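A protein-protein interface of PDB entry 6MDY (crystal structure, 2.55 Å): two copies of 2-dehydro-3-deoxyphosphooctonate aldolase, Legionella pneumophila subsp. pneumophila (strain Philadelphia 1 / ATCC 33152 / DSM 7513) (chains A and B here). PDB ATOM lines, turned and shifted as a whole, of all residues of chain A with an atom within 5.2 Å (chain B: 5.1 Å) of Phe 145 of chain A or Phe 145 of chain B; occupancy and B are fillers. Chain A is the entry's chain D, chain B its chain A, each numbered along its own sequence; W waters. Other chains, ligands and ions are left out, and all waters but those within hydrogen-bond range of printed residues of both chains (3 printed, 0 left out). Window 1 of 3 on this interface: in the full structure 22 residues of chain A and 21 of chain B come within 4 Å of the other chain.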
ATOM      1  N   ALA A 119     -25.931  28.546 -21.775  1.00  0.00           N
ATOM      2  CA  ALA A 119     -25.830  28.805 -20.340  1.00  0.00           C
ATOM      3  C   ALA A 119     -24.428  29.257 -19.934  1.00  0.00           C
ATOM      4  O   ALA A 119     -24.275  30.094 -19.036  1.00  0.00           O
ATOM      5  CB  ALA A 119     -26.245  27.558 -19.558  1.00  0.00           C
ATOM      6  N   PHE A 120     -23.390  28.718 -20.580  1.00  0.00           N
ATOM      7  CA  PHE A 120     -22.037  29.042 -20.148  1.00  0.00           C
ATOM      8  C   PHE A 120     -21.613  30.459 -20.527  1.00  0.00           C
ATOM      9  O   PHE A 120     -20.560  30.916 -20.067  1.00  0.00           O
ATOM     10  CB  PHE A 120     -21.046  28.007 -20.702  1.00  0.00           C
ATOM     11  CG  PHE A 120     -20.755  28.150 -22.172  1.00  0.00           C
ATOM     12  CD1 PHE A 120     -21.568  27.545 -23.116  1.00  0.00           C
ATOM     13  CD2 PHE A 120     -19.648  28.866 -22.608  1.00  0.00           C
ATOM     14  CE1 PHE A 120     -21.295  27.664 -24.481  1.00  0.00           C
ATOM     15  CE2 PHE A 120     -19.371  28.991 -23.974  1.00  0.00           C
ATOM     16  CZ  PHE A 120     -20.195  28.388 -24.909  1.00  0.00           C
ATOM     17  N   CYS A 122     -23.764  33.190 -20.020  1.00  0.00           N
ATOM     18  CA  CYS A 122     -24.718  34.128 -19.430  1.00  0.00           C
ATOM     19  C   CYS A 122     -24.037  35.302 -18.728  1.00  0.00           C
ATOM     20  O   CYS A 122     -24.621  36.385 -18.638  1.00  0.00           O
ATOM     21  CB  CYS A 122     -25.647  33.398 -18.451  1.00  0.00           C
ATOM     22  SG  CYS A 122     -24.823  32.687 -16.987  1.00  0.00           S
ATOM     23  N   ARG A 123     -22.816  35.126 -18.229  1.00  0.00           N
ATOM     24  CA  ARG A 123     -22.113  36.220 -17.562  1.00  0.00           C
ATOM     25  C   ARG A 123     -21.278  37.086 -18.506  1.00  0.00           C
ATOM     26  O   ARG A 123     -20.630  38.028 -18.040  1.00  0.00           O
ATOM     27  CB  ARG A 123     -21.221  35.678 -16.446  1.00  0.00           C
ATOM     28  CG  ARG A 123     -21.971  35.351 -15.171  1.00  0.00           C
ATOM     29  CD  ARG A 123     -20.992  35.091 -14.051  1.00  0.00           C
ATOM     30  NE  ARG A 123     -21.649  34.897 -12.766  1.00  0.00           N
ATOM     31  CZ  ARG A 123     -21.308  33.957 -11.894  1.00  0.00           C
ATOM     32  NH1 ARG A 123     -21.959  33.850 -10.742  1.00  0.00           N
ATOM     33  NH2 ARG A 123     -20.315  33.125 -12.179  1.00  0.00           N
ATOM     34  N   GLY A 143     -27.085  30.147 -16.508  1.00  0.00           N
ATOM     35  CA  GLY A 143     -25.993  29.244 -16.201  1.00  0.00           C
ATOM     36  C   GLY A 143     -26.241  28.479 -14.914  1.00  0.00           C
ATOM     37  O   GLY A 143     -26.803  29.002 -13.948  1.00  0.00           O
ATOM     38  N   GLN A 144     -25.797  27.216 -14.903  1.00  0.00           N
ATOM     39  CA  GLN A 144     -25.941  26.363 -13.722  1.00  0.00           C
ATOM     40  C   GLN A 144     -25.182  26.890 -12.520  1.00  0.00           C
ATOM     41  O   GLN A 144     -25.327  26.323 -11.435  1.00  0.00           O
ATOM     42  CB  GLN A 144     -25.495  24.932 -14.015  1.00  0.00           C
ATOM     43  CG  GLN A 144     -24.069  24.805 -14.463  1.00  0.00           C
ATOM     44  CD  GLN A 144     -23.940  24.805 -15.967  1.00  0.00           C
ATOM     45  OE1 GLN A 144     -24.427  25.715 -16.652  1.00  0.00           O
ATOM     46  NE2 GLN A 144     -23.294  23.771 -16.498  1.00  0.00           N
ATOM     47  N   PHE A 145     -24.344  27.911 -12.700  1.00  0.00           N
ATOM     48  CA  PHE A 145     -23.573  28.541 -11.634  1.00  0.00           C
ATOM     49  C   PHE A 145     -24.185  29.862 -11.174  1.00  0.00           C
ATOM     50  O   PHE A 145     -23.556  30.596 -10.407  1.00  0.00           O
ATOM     51  CB  PHE A 145     -22.131  28.775 -12.101  1.00  0.00           C
ATOM     52  CG  PHE A 145     -22.037  29.314 -13.510  1.00  0.00           C
ATOM     53  CD1 PHE A 145     -22.079  30.681 -13.752  1.00  0.00           C
ATOM     54  CD2 PHE A 145     -21.932  28.450 -14.595  1.00  0.00           C
ATOM     55  CE1 PHE A 145     -22.003  31.171 -15.049  1.00  0.00           C
ATOM     56  CE2 PHE A 145     -21.851  28.937 -15.892  1.00  0.00           C
ATOM     57  CZ  PHE A 145     -21.887  30.292 -16.120  1.00  0.00           C
ATOM     58  N   LEU A 146     -25.391  30.184 -11.623  1.00  0.00           N
ATOM     59  CA  LEU A 146     -26.016  31.463 -11.323  1.00  0.00           C
ATOM     60  C   LEU A 146     -27.125  31.286 -10.299  1.00  0.00           C
ATOM     61  O   LEU A 146     -27.889  30.318 -10.350  1.00  0.00           O
ATOM     62  CB  LEU A 146     -26.590  32.110 -12.584  1.00  0.00           C
ATOM     63  CG  LEU A 146     -25.721  33.172 -13.256  1.00  0.00           C
ATOM     64  CD1 LEU A 146     -24.686  32.530 -14.131  1.00  0.00           C
ATOM     65  CD2 LEU A 146     -26.608  34.085 -14.072  1.00  0.00           C
ATOM     66  N   ALA A 147     -27.185  32.193  -9.373  1.00  0.00           N
ATOM     67  CA  ALA A 147     -28.348  32.298  -8.523  1.00  0.00           C
ATOM     68  C   ALA A 147     -29.453  33.048  -9.270  1.00  0.00           C
ATOM     69  O   ALA A 147     -29.165  33.857 -10.156  1.00  0.00           O
ATOM     70  CB  ALA A 147     -27.994  33.027  -7.229  1.00  0.00           C
ATOM     71  N   GLU A 150     -29.208  36.752  -9.710  1.00  0.00           N
ATOM     72  CA  GLU A 150     -28.213  37.237 -10.662  1.00  0.00           C
ATOM     73  C   GLU A 150     -28.756  37.244 -12.081  1.00  0.00           C
ATOM     74  O   GLU A 150     -28.259  38.001 -12.921  1.00  0.00           O
ATOM     75  CB  GLU A 150     -26.947  36.377 -10.637  1.00  0.00           C
ATOM     76  CG  GLU A 150     -26.127  36.426  -9.365  1.00  0.00           C
ATOM     77  CD  GLU A 150     -24.940  35.472  -9.431  1.00  0.00           C
ATOM     78  OE1 GLU A 150     -25.101  34.283  -9.071  1.00  0.00           O
ATOM     79  OE2 GLU A 150     -23.849  35.906  -9.863  1.00  0.00           O
ATOM     80  N   VAL A 173     -29.470  24.115 -11.639  1.00  0.00           N
ATOM     81  CA  VAL A 173     -28.286  24.655 -10.995  1.00  0.00           C
ATOM     82  C   VAL A 173     -27.480  23.509 -10.408  1.00  0.00           C
ATOM     83  O   VAL A 173     -28.019  22.466 -10.019  1.00  0.00           O
ATOM     84  CB  VAL A 173     -28.625  25.709  -9.917  1.00  0.00           C
ATOM     85  CG1 VAL A 173     -28.986  27.027 -10.587  1.00  0.00           C
ATOM     86  CG2 VAL A 173     -29.749  25.222  -9.033  1.00  0.00           C
ATOM     87  N   SER A 174     -26.162  23.703 -10.392  1.00  0.00           N
ATOM     88  CA  SER A 174     -25.242  22.689  -9.906  1.00  0.00           C
ATOM     89  C   SER A 174     -25.570  22.308  -8.472  1.00  0.00           C
ATOM     90  O   SER A 174     -25.824  23.170  -7.626  1.00  0.00           O
ATOM     91  CB  SER A 174     -23.808  23.206  -9.981  1.00  0.00           C
ATOM     92  OG  SER A 174     -23.462  23.542 -11.310  1.00  0.00           O
ATOM     93  N   ALA B 119     -12.437  29.884 -16.881  1.00  0.00           N
ATOM     94  CA  ALA B 119     -13.155  28.736 -16.328  1.00  0.00           C
ATOM     95  C   ALA B 119     -14.444  28.442 -17.091  1.00  0.00           C
ATOM     96  O   ALA B 119     -14.797  27.275 -17.300  1.00  0.00           O
ATOM     97  CB  ALA B 119     -13.454  28.979 -14.847  1.00  0.00           C
ATOM     98  N   PHE B 120     -15.147  29.480 -17.544  1.00  0.00           N
ATOM     99  CA  PHE B 120     -16.442  29.259 -18.175  1.00  0.00           C
ATOM    100  C   PHE B 120     -16.325  28.647 -19.569  1.00  0.00           C
ATOM    101  O   PHE B 120     -17.352  28.258 -20.136  1.00  0.00           O
ATOM    102  CB  PHE B 120     -17.235  30.578 -18.225  1.00  0.00           C
ATOM    103  CG  PHE B 120     -16.710  31.568 -19.227  1.00  0.00           C
ATOM    104  CD1 PHE B 120     -15.715  32.470 -18.874  1.00  0.00           C
ATOM    105  CD2 PHE B 120     -17.212  31.603 -20.528  1.00  0.00           C
ATOM    106  CE1 PHE B 120     -15.219  33.387 -19.804  1.00  0.00           C
ATOM    107  CE2 PHE B 120     -16.729  32.517 -21.455  1.00  0.00           C
ATOM    108  CZ  PHE B 120     -15.726  33.408 -21.093  1.00  0.00           C
ATOM    109  N   CYS B 122     -14.093  25.980 -20.208  1.00  0.00           N
ATOM    110  CA  CYS B 122     -13.351  24.728 -20.082  1.00  0.00           C
ATOM    111  C   CYS B 122     -14.014  23.579 -20.839  1.00  0.00           C
ATOM    112  O   CYS B 122     -13.335  22.613 -21.203  1.00  0.00           O
ATOM    113  CB  CYS B 122     -13.172  24.370 -18.601  1.00  0.00           C
ATOM    114  SG  CYS B 122     -14.712  24.093 -17.710  1.00  0.00           S
ATOM    115  N   ARG B 123     -15.328  23.637 -21.058  1.00  0.00           N
ATOM    116  CA  ARG B 123     -16.006  22.595 -21.825  1.00  0.00           C
ATOM    117  C   ARG B 123     -16.060  22.862 -23.328  1.00  0.00           C
ATOM    118  O   ARG B 123     -16.578  22.016 -24.065  1.00  0.00           O
ATOM    119  CB  ARG B 123     -17.431  22.383 -21.314  1.00  0.00           C
ATOM    120  CG  ARG B 123     -17.541  21.609 -20.010  1.00  0.00           C
ATOM    121  CD  ARG B 123     -18.972  21.152 -19.831  1.00  0.00           C
ATOM    122  NE  ARG B 123     -19.219  20.565 -18.525  1.00  0.00           N
ATOM    123  CZ  ARG B 123     -20.312  20.812 -17.810  1.00  0.00           C
ATOM    124  NH1 ARG B 123     -21.238  21.636 -18.292  1.00  0.00           N
ATOM    125  NH2 ARG B 123     -20.480  20.244 -16.619  1.00  0.00           N
ATOM    126  N   GLY B 143     -13.792  24.780 -14.597  1.00  0.00           N
ATOM    127  CA  GLY B 143     -15.028  25.480 -14.312  1.00  0.00           C
ATOM    128  C   GLY B 143     -15.592  25.111 -12.952  1.00  0.00           C
ATOM    129  O   GLY B 143     -15.454  23.985 -12.473  1.00  0.00           O
ATOM    130  N   GLN B 144     -16.245  26.088 -12.317  1.00  0.00           N
ATOM    131  CA  GLN B 144     -16.911  25.876 -11.036  1.00  0.00           C
ATOM    132  C   GLN B 144     -18.023  24.843 -11.121  1.00  0.00           C
ATOM    133  O   GLN B 144     -18.516  24.396 -10.077  1.00  0.00           O
ATOM    134  CB  GLN B 144     -17.471  27.199 -10.521  1.00  0.00           C
ATOM    135  CG  GLN B 144     -18.136  28.030 -11.600  1.00  0.00           C
ATOM    136  CD  GLN B 144     -17.158  28.986 -12.251  1.00  0.00           C
ATOM    137  OE1 GLN B 144     -16.693  29.929 -11.613  1.00  0.00           O
ATOM    138  NE2 GLN B 144     -16.813  28.730 -13.515  1.00  0.00           N
ATOM    139  N   PHE B 145     -18.415  24.455 -12.333  1.00  0.00           N
ATOM    140  CA  PHE B 145     -19.458  23.475 -12.597  1.00  0.00           C
ATOM    141  C   PHE B 145     -18.885  22.111 -12.945  1.00  0.00           C
ATOM    142  O   PHE B 145     -19.635  21.223 -13.365  1.00  0.00           O
ATOM    143  CB  PHE B 145     -20.350  23.970 -13.741  1.00  0.00           C
ATOM    144  CG  PHE B 145     -19.574  24.607 -14.869  1.00  0.00           C
ATOM    145  CD1 PHE B 145     -19.228  25.955 -14.823  1.00  0.00           C
ATOM    146  CD2 PHE B 145     -19.169  23.855 -15.965  1.00  0.00           C
ATOM    147  CE1 PHE B 145     -18.500  26.543 -15.861  1.00  0.00           C
ATOM    148  CE2 PHE B 145     -18.450  24.435 -17.013  1.00  0.00           C
ATOM    149  CZ  PHE B 145     -18.112  25.778 -16.960  1.00  0.00           C
ATOM    150  N   LEU B 146     -17.576  21.930 -12.791  1.00  0.00           N
ATOM    151  CA  LEU B 146     -16.889  20.706 -13.180  1.00  0.00           C
ATOM    152  C   LEU B 146     -16.475  19.891 -11.964  1.00  0.00           C
ATOM    153  O   LEU B 146     -16.034  20.442 -10.947  1.00  0.00           O
ATOM    154  CB  LEU B 146     -15.644  21.004 -14.021  1.00  0.00           C
ATOM    155  CG  LEU B 146     -15.747  20.593 -15.491  1.00  0.00           C
ATOM    156  CD1 LEU B 146     -16.750  21.467 -16.214  1.00  0.00           C
ATOM    157  CD2 LEU B 146     -14.388  20.668 -16.145  1.00  0.00           C
ATOM    158  N   ALA B 147     -16.639  18.588 -12.071  1.00  0.00           N
ATOM    159  CA  ALA B 147     -16.041  17.681 -11.110  1.00  0.00           C
ATOM    160  C   ALA B 147     -14.572  17.457 -11.469  1.00  0.00           C
ATOM    161  O   ALA B 147     -14.199  17.531 -12.643  1.00  0.00           O
ATOM    162  CB  ALA B 147     -16.792  16.359 -11.092  1.00  0.00           C
ATOM    163  N   GLU B 150     -13.514  15.256 -14.314  1.00  0.00           N
ATOM    164  CA  GLU B 150     -13.804  15.709 -15.664  1.00  0.00           C
ATOM    165  C   GLU B 150     -12.624  16.446 -16.284  1.00  0.00           C
ATOM    166  O   GLU B 150     -12.568  16.570 -17.511  1.00  0.00           O
ATOM    167  CB  GLU B 150     -15.044  16.601 -15.673  1.00  0.00           C
ATOM    168  CG  GLU B 150     -16.351  15.889 -15.346  1.00  0.00           C
ATOM    169  CD  GLU B 150     -17.540  16.830 -15.416  1.00  0.00           C
ATOM    170  OE1 GLU B 150     -18.147  16.948 -16.503  1.00  0.00           O
ATOM    171  OE2 GLU B 150     -17.855  17.469 -14.389  1.00  0.00           O
ATOM    172  N   SER B 174     -18.870  25.377  -7.323  1.00  0.00           N
ATOM    173  CA  SER B 174     -20.095  25.991  -6.826  1.00  0.00           C
ATOM    174  C   SER B 174     -20.619  25.242  -5.609  1.00  0.00           C
ATOM    175  O   SER B 174     -20.659  24.011  -5.583  1.00  0.00           O
ATOM    176  CB  SER B 174     -21.161  26.024  -7.920  1.00  0.00           C
ATOM    177  OG  SER B 174     -20.767  26.882  -8.967  1.00  0.00           O
HETATM  178  O   HOH W   1     -23.598  22.893  -5.580  1.00  0.00           O
HETATM  179  O   HOH W   2     -22.248  21.443 -12.438  1.00  0.00           O
HETATM  180  O   HOH W   3     -23.280  21.148 -15.382  1.00  0.00           O
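O of Gln 144 of chain A lies within hydrogen-bond range of N of Ser 174 of chain A (2.9 Å). The backbone NH (N) of Ser 174 of chain B is in hydrogen-bond range of the backbone carbonyl oxygen (O) of Gln 144 of chain B.
Phe 145 of chain A touches two residues of chain B. Of the printed residues of chain A, Ser 174 of chain B touches Phe 145. Of the printed residues of chain A, Phe 120 of chain B touches Phe 120. Printed residues of chain B within 4 Å of Gln 144 of chain A: Arg 123 and Phe 145. Val 173 of chain A touches none of the printed residues of chain B. The nearest residue of chain B that does not touch Phe 145 of chain A is Gln 144 of chain B (4.1 Å). The nearest printed residue of chain A that does not touch Phe 145 of chain B is Phe 120 of chain A (5.3 Å). The nearest printed residue of chain B that does not touch Ser 174 of chain A is Ser 174 of chain B (4.4 Å).
Water W2 lies within hydrogen-bond range of OG of Ser 174 of chain A (2.7 Å) and O of Phe 145 of chain B (2.8 Å). Water W3 bridges NE2 of Gln 144 of chain A (2.9 Å) and NH2 of Arg 123 of chain B (3.2 Å). Water W1 bridges O of Ser 174 of chain A (3.0 Å) and O of Ser 174 of chain B (3.1 Å).
NH1 of Arg 123 of chain B sits close to NE2 of Gln 144 of chain A (3.5 Å).
Phe 120 of chain B touches its own counterpart, Phe 120 of chain A. Gln 144 of chain A touches Arg 123 of chain B, but with the chains exchanged Arg 123 of chain A does not touch Gln 144 of chain B (4.9 Å). Phe 145 of chain B touches its own counterpart, Phe 145 of chain A. Phe 145 of chain A touches Ser 174 of chain B, and with the chains exchanged Ser 174 of chain A touches Phe 145 of chain B.
Of the 12 printed residues of chain A, 4 touch a printed residue of chain B. Printed residues of chain A that touch a printed residue of chain B: Phe 120, Gln 144, Phe 145 and Ser 174. Hydrophobic or aromatic side chains of chain A within 4 Å of the printed part of chain B: Phe 120 and Phe 145. Along chain B the printed residues that touch a printed residue of chain A span positions 120 to 174.
Among the printed residues, merely in contact across the chains: Phe 120 of chain A with Phe 120 of chain B (3.4 Å), Phe 145 of chain A with Phe 145 of chain B (3.7 Å), Gln 144 of chain A with Phe 145 of chain B (3.9 Å), Phe 145 of chain A with Ser 174 of chain B (3.9 Å) and Ser 174 of chain A with Phe 145 of chain B (3.97 Å).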
